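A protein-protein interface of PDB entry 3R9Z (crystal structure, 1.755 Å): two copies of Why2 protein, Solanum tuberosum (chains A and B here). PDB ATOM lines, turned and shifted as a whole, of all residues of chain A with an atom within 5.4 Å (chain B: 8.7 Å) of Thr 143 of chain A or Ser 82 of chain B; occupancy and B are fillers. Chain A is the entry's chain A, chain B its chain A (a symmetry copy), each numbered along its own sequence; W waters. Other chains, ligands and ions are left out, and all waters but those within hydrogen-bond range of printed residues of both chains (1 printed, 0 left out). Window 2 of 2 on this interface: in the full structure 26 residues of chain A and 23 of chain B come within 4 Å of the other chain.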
ATOM      1  N   GLY A 117      -2.181 -35.345  16.622  1.00  0.00           N
ATOM      2  CA  GLY A 117      -0.776 -35.301  16.243  1.00  0.00           C
ATOM      3  C   GLY A 117      -0.216 -33.897  16.422  1.00  0.00           C
ATOM      4  O   GLY A 117       0.689 -33.476  15.693  1.00  0.00           O
ATOM      5  N   SER A 118      -0.777 -33.169  17.385  1.00  0.00           N
ATOM      6  CA  SER A 118      -0.344 -31.815  17.702  1.00  0.00           C
ATOM      7  C   SER A 118       0.491 -31.809  18.977  1.00  0.00           C
ATOM      8  O   SER A 118       0.750 -30.739  19.547  1.00  0.00           O
ATOM      9  CB  SER A 118      -1.558 -30.903  17.890  1.00  0.00           C
ATOM     10  OG  SER A 118      -2.293 -31.255  19.057  1.00  0.00           O
ATOM     11  N   GLY A 119       0.888 -33.002  19.423  1.00  0.00           N
ATOM     12  CA  GLY A 119       1.647 -33.165  20.663  1.00  0.00           C
ATOM     13  C   GLY A 119       1.528 -34.575  21.233  1.00  0.00           C
ATOM     14  O   GLY A 119       1.070 -35.499  20.546  1.00  0.00           O
ATOM     15  N   VAL A 141       2.261 -32.469  26.214  1.00  0.00           N
ATOM     16  CA  VAL A 141       3.302 -31.616  25.627  1.00  0.00           C
ATOM     17  C   VAL A 141       2.970 -31.332  24.158  1.00  0.00           C
ATOM     18  O   VAL A 141       2.661 -32.247  23.402  1.00  0.00           O
ATOM     19  CB  VAL A 141       4.727 -32.249  25.730  1.00  0.00           C
ATOM     20  CG1 VAL A 141       5.181 -32.367  27.215  1.00  0.00           C
ATOM     21  CG2 VAL A 141       4.766 -33.588  25.059  1.00  0.00           C
ATOM     22  N   THR A 142       3.018 -30.063  23.755  1.00  0.00           N
ATOM     23  CA  THR A 142       2.724 -29.687  22.385  1.00  0.00           C
ATOM     24  C   THR A 142       3.860 -30.120  21.454  1.00  0.00           C
ATOM     25  O   THR A 142       4.928 -30.517  21.925  1.00  0.00           O
ATOM     26  CB  THR A 142       2.522 -28.159  22.250  1.00  0.00           C
ATOM     27  OG1 THR A 142       3.765 -27.507  22.525  1.00  0.00           O
ATOM     28  CG2 THR A 142       1.477 -27.668  23.250  1.00  0.00           C
ATOM     29  N   THR A 143       3.608 -30.056  20.143  1.00  0.00           N
ATOM     30  CA  THR A 143       4.646 -30.294  19.133  1.00  0.00           C
ATOM     31  C   THR A 143       5.841 -29.394  19.379  1.00  0.00           C
ATOM     32  O   THR A 143       6.977 -29.849  19.343  1.00  0.00           O
ATOM     33  CB  THR A 143       4.129 -30.003  17.713  1.00  0.00           C
ATOM     34  OG1 THR A 143       3.042 -30.890  17.422  1.00  0.00           O
ATOM     35  CG2 THR A 143       5.247 -30.188  16.660  1.00  0.00           C
ATOM     36  N   ALA A 144       5.574 -28.109  19.599  1.00  0.00           N
ATOM     37  CA  ALA A 144       6.639 -27.139  19.870  1.00  0.00           C
ATOM     38  C   ALA A 144       7.452 -27.516  21.109  1.00  0.00           C
ATOM     39  O   ALA A 144       8.684 -27.475  21.090  1.00  0.00           O
ATOM     40  CB  ALA A 144       6.054 -25.723  20.015  1.00  0.00           C
ATOM     41  N   GLU A 145       6.764 -27.883  22.191  1.00  0.00           N
ATOM     42  CA  GLU A 145       7.444 -28.307  23.418  1.00  0.00           C
ATOM     43  C   GLU A 145       8.251 -29.598  23.214  1.00  0.00           C
ATOM     44  O   GLU A 145       9.362 -29.723  23.717  1.00  0.00           O
ATOM     45  CB  GLU A 145       6.440 -28.459  24.575  1.00  0.00           C
ATOM     46  CG  GLU A 145       5.872 -27.126  25.086  1.00  0.00           C
ATOM     47  CD  GLU A 145       4.601 -27.263  25.925  1.00  0.00           C
ATOM     48  OE1 GLU A 145       3.917 -28.306  25.840  1.00  0.00           O
ATOM     49  OE2 GLU A 145       4.276 -26.309  26.672  1.00  0.00           O
ATOM     50  N   PHE A 146       7.699 -30.553  22.469  1.00  0.00           N
ATOM     51  CA  PHE A 146       8.417 -31.798  22.207  1.00  0.00           C
ATOM     52  C   PHE A 146       9.603 -31.505  21.273  1.00  0.00           C
ATOM     53  O   PHE A 146      10.621 -32.169  21.360  1.00  0.00           O
ATOM     54  CB  PHE A 146       7.486 -32.888  21.630  1.00  0.00           C
ATOM     55  CG  PHE A 146       8.094 -34.287  21.628  1.00  0.00           C
ATOM     56  CD1 PHE A 146       8.222 -35.008  22.809  1.00  0.00           C
ATOM     57  CD2 PHE A 146       8.545 -34.863  20.445  1.00  0.00           C
ATOM     58  CE1 PHE A 146       8.778 -36.296  22.813  1.00  0.00           C
ATOM     59  CE2 PHE A 146       9.101 -36.143  20.442  1.00  0.00           C
ATOM     60  CZ  PHE A 146       9.217 -36.857  21.628  1.00  0.00           C
ATOM     61  N   ALA A 147       9.480 -30.496  20.407  1.00  0.00           N
ATOM     62  CA  ALA A 147      10.599 -30.150  19.522  1.00  0.00           C
ATOM     63  C   ALA A 147      11.750 -29.564  20.324  1.00  0.00           C
ATOM     64  O   ALA A 147      12.921 -29.799  19.995  1.00  0.00           O
ATOM     65  CB  ALA A 147      10.174 -29.206  18.406  1.00  0.00           C
ATOM     66  N   VAL A 148      11.430 -28.795  21.365  1.00  0.00           N
ATOM     67  CA  VAL A 148      12.464 -28.314  22.277  1.00  0.00           C
ATOM     68  C   VAL A 148      13.152 -29.534  22.894  1.00  0.00           C
ATOM     69  O   VAL A 148      14.378 -29.618  22.931  1.00  0.00           O
ATOM     70  CB  VAL A 148      11.884 -27.399  23.399  1.00  0.00           C
ATOM     71  CG1 VAL A 148      12.967 -27.055  24.442  1.00  0.00           C
ATOM     72  CG2 VAL A 148      11.293 -26.116  22.802  1.00  0.00           C
ATOM     73  N   ARG A 150      13.372 -32.736  21.794  1.00  0.00           N
ATOM     74  CA  ARG A 150      14.187 -33.429  20.791  1.00  0.00           C
ATOM     75  C   ARG A 150      15.506 -32.702  20.504  1.00  0.00           C
ATOM     76  O   ARG A 150      16.572 -33.316  20.487  1.00  0.00           O
ATOM     77  CB  ARG A 150      13.415 -33.602  19.480  1.00  0.00           C
ATOM     78  CG  ARG A 150      14.174 -34.407  18.441  1.00  0.00           C
ATOM     79  CD  ARG A 150      13.438 -34.460  17.106  1.00  0.00           C
ATOM     80  NE  ARG A 150      12.047 -34.862  17.278  1.00  0.00           N
ATOM     81  CZ  ARG A 150      11.010 -34.053  17.101  1.00  0.00           C
ATOM     82  NH1 ARG A 150      11.191 -32.792  16.724  1.00  0.00           N
ATOM     83  NH2 ARG A 150       9.784 -34.513  17.282  1.00  0.00           N
ATOM     84  N   THR B  75      10.148 -22.238  23.578  1.00  0.00           N
ATOM     85  CA  THR B  75       9.040 -22.991  23.016  1.00  0.00           C
ATOM     86  C   THR B  75       8.622 -22.440  21.648  1.00  0.00           C
ATOM     87  O   THR B  75       8.350 -23.208  20.726  1.00  0.00           O
ATOM     88  CB  THR B  75       7.849 -23.045  24.008  1.00  0.00           C
ATOM     89  OG1 THR B  75       8.258 -23.713  25.211  1.00  0.00           O
ATOM     90  CG2 THR B  75       6.679 -23.778  23.411  1.00  0.00           C
ATOM     91  N   GLU B  76       8.600 -21.117  21.504  1.00  0.00           N
ATOM     92  CA  GLU B  76       8.301 -20.506  20.203  1.00  0.00           C
ATOM     93  C   GLU B  76       9.369 -20.835  19.155  1.00  0.00           C
ATOM     94  O   GLU B  76       9.045 -21.045  17.987  1.00  0.00           O
ATOM     95  CB  GLU B  76       8.061 -18.998  20.345  1.00  0.00           C
ATOM     96  CG  GLU B  76       6.745 -18.686  21.071  1.00  0.00           C
ATOM     97  CD  GLU B  76       6.617 -17.242  21.534  1.00  0.00           C
ATOM     98  OE1 GLU B  76       7.649 -16.610  21.822  1.00  0.00           O
ATOM     99  OE2 GLU B  76       5.468 -16.752  21.646  1.00  0.00           O
ATOM    100  N   VAL B  77      10.632 -20.908  19.574  1.00  0.00           N
ATOM    101  CA  VAL B  77      11.710 -21.375  18.674  1.00  0.00           C
ATOM    102  C   VAL B  77      11.479 -22.841  18.271  1.00  0.00           C
ATOM    103  O   VAL B  77      11.644 -23.223  17.097  1.00  0.00           O
ATOM    104  CB  VAL B  77      13.100 -21.181  19.315  1.00  0.00           C
ATOM    105  CG1 VAL B  77      14.202 -21.795  18.442  1.00  0.00           C
ATOM    106  CG2 VAL B  77      13.367 -19.693  19.544  1.00  0.00           C
ATOM    107  N   GLY B  78      11.057 -23.661  19.235  1.00  0.00           N
ATOM    108  CA  GLY B  78      10.671 -25.038  18.957  1.00  0.00           C
ATOM    109  C   GLY B  78       9.606 -25.125  17.874  1.00  0.00           C
ATOM    110  O   GLY B  78       9.656 -25.995  17.004  1.00  0.00           O
ATOM    111  N   SER B  79       8.636 -24.216  17.934  1.00  0.00           N
ATOM    112  CA  SER B  79       7.602 -24.136  16.926  1.00  0.00           C
ATOM    113  C   SER B  79       8.199 -23.859  15.531  1.00  0.00           C
ATOM    114  O   SER B  79       7.869 -24.542  14.551  1.00  0.00           O
ATOM    115  CB  SER B  79       6.594 -23.053  17.307  1.00  0.00           C
ATOM    116  OG  SER B  79       5.481 -23.086  16.453  1.00  0.00           O
ATOM    117  N   LEU B  80       9.082 -22.872  15.457  1.00  0.00           N
ATOM    118  CA  LEU B  80       9.687 -22.465  14.185  1.00  0.00           C
ATOM    119  C   LEU B  80      10.564 -23.579  13.594  1.00  0.00           C
ATOM    120  O   LEU B  80      10.473 -23.884  12.405  1.00  0.00           O
ATOM    121  CB  LEU B  80      10.482 -21.160  14.375  1.00  0.00           C
ATOM    122  CG  LEU B  80      11.012 -20.409  13.148  1.00  0.00           C
ATOM    123  CD1 LEU B  80      11.183 -18.921  13.464  1.00  0.00           C
ATOM    124  CD2 LEU B  80      12.310 -21.015  12.631  1.00  0.00           C
ATOM    125  N   ILE B  81      11.410 -24.192  14.417  1.00  0.00           N
ATOM    126  CA  ILE B  81      12.329 -25.201  13.884  1.00  0.00           C
ATOM    127  C   ILE B  81      11.653 -26.506  13.468  1.00  0.00           C
ATOM    128  O   ILE B  81      12.204 -27.287  12.682  1.00  0.00           O
ATOM    129  CB  ILE B  81      13.538 -25.467  14.829  1.00  0.00           C
ATOM    130  CG1 ILE B  81      13.091 -26.186  16.098  1.00  0.00           C
ATOM    131  CG2 ILE B  81      14.257 -24.168  15.140  1.00  0.00           C
ATOM    132  CD1 ILE B  81      14.193 -26.287  17.161  1.00  0.00           C
ATOM    133  N   SER B  82      10.443 -26.740  13.952  1.00  0.00           N
ATOM    134  CA  SER B  82       9.747 -27.961  13.590  1.00  0.00           C
ATOM    135  C   SER B  82       8.748 -27.758  12.436  1.00  0.00           C
ATOM    136  O   SER B  82       8.055 -28.690  12.040  1.00  0.00           O
ATOM    137  CB  SER B  82       9.102 -28.625  14.823  1.00  0.00           C
ATOM    138  OG  SER B  82       8.122 -27.810  15.434  1.00  0.00           O
ATOM    139  N   MET B  83       8.706 -26.540  11.890  1.00  0.00           N
ATOM    140  CA  MET B  83       7.826 -26.220  10.768  1.00  0.00           C
ATOM    141  C   MET B  83       8.256 -26.898   9.479  1.00  0.00           C
ATOM    142  O   MET B  83       9.426 -26.858   9.111  1.00  0.00           O
ATOM    143  CB  MET B  83       7.786 -24.711  10.530  1.00  0.00           C
ATOM    144  CG  MET B  83       6.951 -23.961  11.519  1.00  0.00           C
ATOM    145  SD  MET B  83       7.027 -22.217  11.133  1.00  0.00           S
ATOM    146  CE  MET B  83       5.907 -22.139   9.738  1.00  0.00           C
ATOM    147  N   GLY B  84       7.294 -27.510   8.794  1.00  0.00           N
ATOM    148  CA  GLY B  84       7.526 -28.054   7.470  1.00  0.00           C
ATOM    149  C   GLY B  84       7.228 -26.997   6.420  1.00  0.00           C
ATOM    150  O   GLY B  84       6.761 -25.907   6.750  1.00  0.00           O
ATOM    151  N   THR B  85       7.491 -27.336   5.161  1.00  0.00           N
ATOM    152  CA  THR B  85       7.317 -26.431   4.024  1.00  0.00           C
ATOM    153  C   THR B  85       5.960 -25.724   3.994  1.00  0.00           C
ATOM    154  O   THR B  85       5.864 -24.572   3.570  1.00  0.00           O
ATOM    155  CB  THR B  85       7.511 -27.196   2.698  1.00  0.00           C
ATOM    156  OG1 THR B  85       8.773 -27.882   2.721  1.00  0.00           O
ATOM    157  CG2 THR B  85       7.466 -26.242   1.503  1.00  0.00           C
ATOM    158  N   ARG B  86       4.914 -26.425   4.430  1.00  0.00           N
ATOM    159  CA  ARG B  86       3.547 -25.935   4.278  1.00  0.00           C
ATOM    160  C   ARG B  86       2.877 -25.621   5.614  1.00  0.00           C
ATOM    161  O   ARG B  86       1.656 -25.458   5.679  1.00  0.00           O
ATOM    162  CB  ARG B  86       2.710 -26.971   3.523  1.00  0.00           C
ATOM    163  CG  ARG B  86       3.282 -27.353   2.167  1.00  0.00           C
ATOM    164  CD  ARG B  86       3.101 -26.242   1.143  1.00  0.00           C
ATOM    165  NE  ARG B  86       3.679 -26.602  -0.152  1.00  0.00           N
ATOM    166  CZ  ARG B  86       3.441 -25.953  -1.288  1.00  0.00           C
ATOM    167  NH1 ARG B  86       2.620 -24.911  -1.303  1.00  0.00           N
ATOM    168  NH2 ARG B  86       4.014 -26.352  -2.414  1.00  0.00           N
ATOM    169  N   ASP B  87       3.679 -25.528   6.667  1.00  0.00           N
ATOM    170  CA  ASP B  87       3.170 -25.249   8.009  1.00  0.00           C
ATOM    171  C   ASP B  87       3.048 -23.738   8.266  1.00  0.00           C
ATOM    172  O   ASP B  87       3.761 -22.939   7.663  1.00  0.00           O
ATOM    173  CB  ASP B  87       4.076 -25.889   9.071  1.00  0.00           C
ATOM    174  CG  ASP B  87       3.891 -27.405   9.181  1.00  0.00           C
ATOM    175  OD1 ASP B  87       2.767 -27.901   8.957  1.00  0.00           O
ATOM    176  OD2 ASP B  87       4.880 -28.096   9.501  1.00  0.00           O
ATOM    177  N   SER B  88       2.136 -23.363   9.162  1.00  0.00           N
ATOM    178  CA  SER B  88       1.945 -21.968   9.569  1.00  0.00           C
ATOM    179  C   SER B  88       1.992 -21.870  11.085  1.00  0.00           C
ATOM    180  O   SER B  88       1.829 -22.866  11.784  1.00  0.00           O
ATOM    181  CB  SER B  88       0.591 -21.442   9.087  1.00  0.00           C
ATOM    182  OG  SER B  88       0.631 -21.065   7.726  1.00  0.00           O
ATOM    183  N   SER B  89       2.218 -20.671  11.603  1.00  0.00           N
ATOM    184  CA  SER B  89       2.123 -20.473  13.040  1.00  0.00           C
ATOM    185  C   SER B  89       1.878 -19.013  13.364  1.00  0.00           C
ATOM    186  O   SER B  89       2.154 -18.129  12.553  1.00  0.00           O
ATOM    187  CB  SER B  89       3.387 -20.953  13.740  1.00  0.00           C
ATOM    188  OG  SER B  89       4.445 -20.045  13.535  1.00  0.00           O
ATOM    189  N   TYR B 120       8.391 -18.206   2.883  1.00  0.00           N
ATOM    190  CA  TYR B 120       7.317 -17.811   3.793  1.00  0.00           C
ATOM    191  C   TYR B 120       7.127 -16.298   3.796  1.00  0.00           C
ATOM    192  O   TYR B 120       7.923 -15.557   3.218  1.00  0.00           O
ATOM    193  CB  TYR B 120       7.643 -18.256   5.222  1.00  0.00           C
ATOM    194  CG  TYR B 120       7.891 -19.735   5.386  1.00  0.00           C
ATOM    195  CD1 TYR B 120       9.127 -20.292   5.060  1.00  0.00           C
ATOM    196  CD2 TYR B 120       6.898 -20.571   5.872  1.00  0.00           C
ATOM    197  CE1 TYR B 120       9.363 -21.654   5.212  1.00  0.00           C
ATOM    198  CE2 TYR B 120       7.119 -21.940   6.028  1.00  0.00           C
ATOM    199  CZ  TYR B 120       8.354 -22.472   5.694  1.00  0.00           C
ATOM    200  OH  TYR B 120       8.579 -23.820   5.854  1.00  0.00           O
ATOM    201  N   PHE B 146      15.031 -19.254   5.252  1.00  0.00           N
ATOM    202  CA  PHE B 146      14.364 -19.885   6.389  1.00  0.00           C
ATOM    203  C   PHE B 146      15.219 -21.064   6.880  1.00  0.00           C
ATOM    204  O   PHE B 146      15.215 -21.365   8.061  1.00  0.00           O
ATOM    205  CB  PHE B 146      12.924 -20.325   6.038  1.00  0.00           C
ATOM    206  CG  PHE B 146      12.077 -20.700   7.249  1.00  0.00           C
ATOM    207  CD1 PHE B 146      11.581 -19.719   8.101  1.00  0.00           C
ATOM    208  CD2 PHE B 146      11.796 -22.033   7.535  1.00  0.00           C
ATOM    209  CE1 PHE B 146      10.799 -20.058   9.215  1.00  0.00           C
ATOM    210  CE2 PHE B 146      11.021 -22.376   8.642  1.00  0.00           C
ATOM    211  CZ  PHE B 146      10.524 -21.387   9.482  1.00  0.00           C
ATOM    212  N   ARG B 150      16.240 -21.814  10.674  1.00  0.00           N
ATOM    213  CA  ARG B 150      16.063 -23.096  11.364  1.00  0.00           C
ATOM    214  C   ARG B 150      17.378 -23.637  11.939  1.00  0.00           C
ATOM    215  O   ARG B 150      17.438 -24.043  13.098  1.00  0.00           O
ATOM    216  CB  ARG B 150      15.457 -24.145  10.429  1.00  0.00           C
ATOM    217  CG  ARG B 150      15.155 -25.461  11.123  1.00  0.00           C
ATOM    218  CD  ARG B 150      14.666 -26.526  10.146  1.00  0.00           C
ATOM    219  NE  ARG B 150      13.582 -26.027   9.308  1.00  0.00           N
ATOM    220  CZ  ARG B 150      13.696 -25.784   8.008  1.00  0.00           C
ATOM    221  NH1 ARG B 150      14.841 -26.013   7.374  1.00  0.00           N
ATOM    222  NH2 ARG B 150      12.652 -25.332   7.335  1.00  0.00           N
ATOM    223  N   PHE B 153      18.789 -21.038  14.583  1.00  0.00           N
ATOM    224  CA  PHE B 153      17.954 -20.999  15.791  1.00  0.00           C
ATOM    225  C   PHE B 153      18.095 -22.330  16.543  1.00  0.00           C
ATOM    226  O   PHE B 153      18.088 -22.343  17.774  1.00  0.00           O
ATOM    227  CB  PHE B 153      16.470 -20.752  15.489  1.00  0.00           C
ATOM    228  CG  PHE B 153      16.145 -19.371  14.952  1.00  0.00           C
ATOM    229  CD1 PHE B 153      17.139 -18.519  14.478  1.00  0.00           C
ATOM    230  CD2 PHE B 153      14.819 -18.944  14.907  1.00  0.00           C
ATOM    231  CE1 PHE B 153      16.810 -17.256  13.965  1.00  0.00           C
ATOM    232  CE2 PHE B 153      14.486 -17.679  14.411  1.00  0.00           C
ATOM    233  CZ  PHE B 153      15.481 -16.842  13.936  1.00  0.00           C
ATOM    234  N   SER B 154      18.216 -23.445  15.811  1.00  0.00           N
ATOM    235  CA  SER B 154      18.413 -24.762  16.449  1.00  0.00           C
ATOM    236  C   SER B 154      19.747 -24.827  17.174  1.00  0.00           C
ATOM    237  O   SER B 154      19.844 -25.391  18.268  1.00  0.00           O
ATOM    238  CB  SER B 154      18.337 -25.920  15.444  1.00  0.00           C
ATOM    239  OG  SER B 154      17.001 -26.137  15.022  1.00  0.00           O
ATOM    240  N   LEU B 157      19.309 -22.762  20.361  1.00  0.00           N
ATOM    241  CA  LEU B 157      18.295 -23.152  21.344  1.00  0.00           C
ATOM    242  C   LEU B 157      18.866 -23.653  22.681  1.00  0.00           C
ATOM    243  O   LEU B 157      18.465 -23.159  23.732  1.00  0.00           O
ATOM    244  CB  LEU B 157      17.292 -24.151  20.751  1.00  0.00           C
ATOM    245  CG  LEU B 157      16.172 -24.595  21.698  1.00  0.00           C
ATOM    246  CD1 LEU B 157      15.311 -23.404  22.103  1.00  0.00           C
ATOM    247  CD2 LEU B 157      15.324 -25.684  21.002  1.00  0.00           C
HETATM  248  O   HOH W   1       6.096 -24.154  27.000  1.00  0.00           O
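2 positions are printed for both chains.
Of the 8 pairs that touch across the chains among the printed residues, none has its exchanged pair printed and touching as well.
Thr 143 of chain A touches Ser 82 of chain B (CG2 to OG, 3.9 Å).
Ala 144 of chain A touches Thr 75 of chain B.
Ala 144 of chain A touches Gly 78 of chain B.
Ser 79 of chain B touches Ala 144 of chain A.
Thr 75 of chain B touches Glu 145 of chain A (CG2 to CG, 3.8 Å).
Gly 78 of chain B touches Ala 147 of chain A.
Ala 147 of chain A touches Ser 82 of chain B (CB to CB, 3.8 Å).
Thr 75 of chain B touches Val 148 of chain A.
No residue of chain B comes within 4 Å of Thr 142 of chain A.
Of chain B, only Ser 82 comes within 4 Å of Thr 143 of chain A.
Printed residues of chain B within 4 Å of Glu 145 of chain A: Thr 75.
Of the printed residues of chain B, Ala 147 of chain A touches Gly 78 (3.5 Å) and Ser 82 (3.8 Å).
Printed residues of chain A within 4 Å of Gly 78 of chain B: Ala 144 (3.8 Å) and Ala 147 (3.5 Å).
Printed residues of chain A within 4 Å of Ser 79 of chain B: Ala 144.
Ile 81 of chain B touches none of the printed residues of chain A.
Printed residues of chain A within 4 Å of Ser 82 of chain B: Thr 143 (3.9 Å) and Ala 147 (3.8 Å).
Tyr 120 of chain B touches none of the printed residues of chain A.
The nearest residue of chain B that does not touch Thr 143 of chain A is Gly 78 of chain B (5.2 Å).
The nearest residue of chain A that does not touch Ser 82 of chain B is Ala 144 of chain A (4.7 Å).
Water W1 bridges the side-chain carboxylate of Glu 145 of chain A (2.8 Å) and the side-chain hydroxyl of Thr 75 of chain B (2.8 Å).
Of the 12 printed residues of chain A, 5 touch a printed residue of chain B.
Of the 21 printed residues of chain B, 4 touch a printed residue of chain A.
Among the printed residues, 8 pairs touch across the chains.
Among the printed residues, no Asp or Glu carboxylate lies within 4 Å of a Lys or Arg side-chain nitrogen of the other chain.
O of Ser 118 of chain A lies within hydrogen-bond range of N of Thr 143 of chain A (3.0 Å).
The backbone NH (N) of Ala 144 of chain A sits close to the side-chain hydroxyl (OG1) of Thr 142 of chain A.
N of Thr 142 of chain A sits at hydrogen-bond distance from OE1 of Glu 145 of chain A (2.9 Å).
The backbone carbonyl oxygen (O) of Gly 78 of chain B is in hydrogen-bond range of the side-chain hydroxyl (OG) of Ser 82 of chain B, 2.8 Å away.
OG of Ser 82 of chain B is in hydrogen-bond range of O of Ser 79 of chain B, at 3.4 Å.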
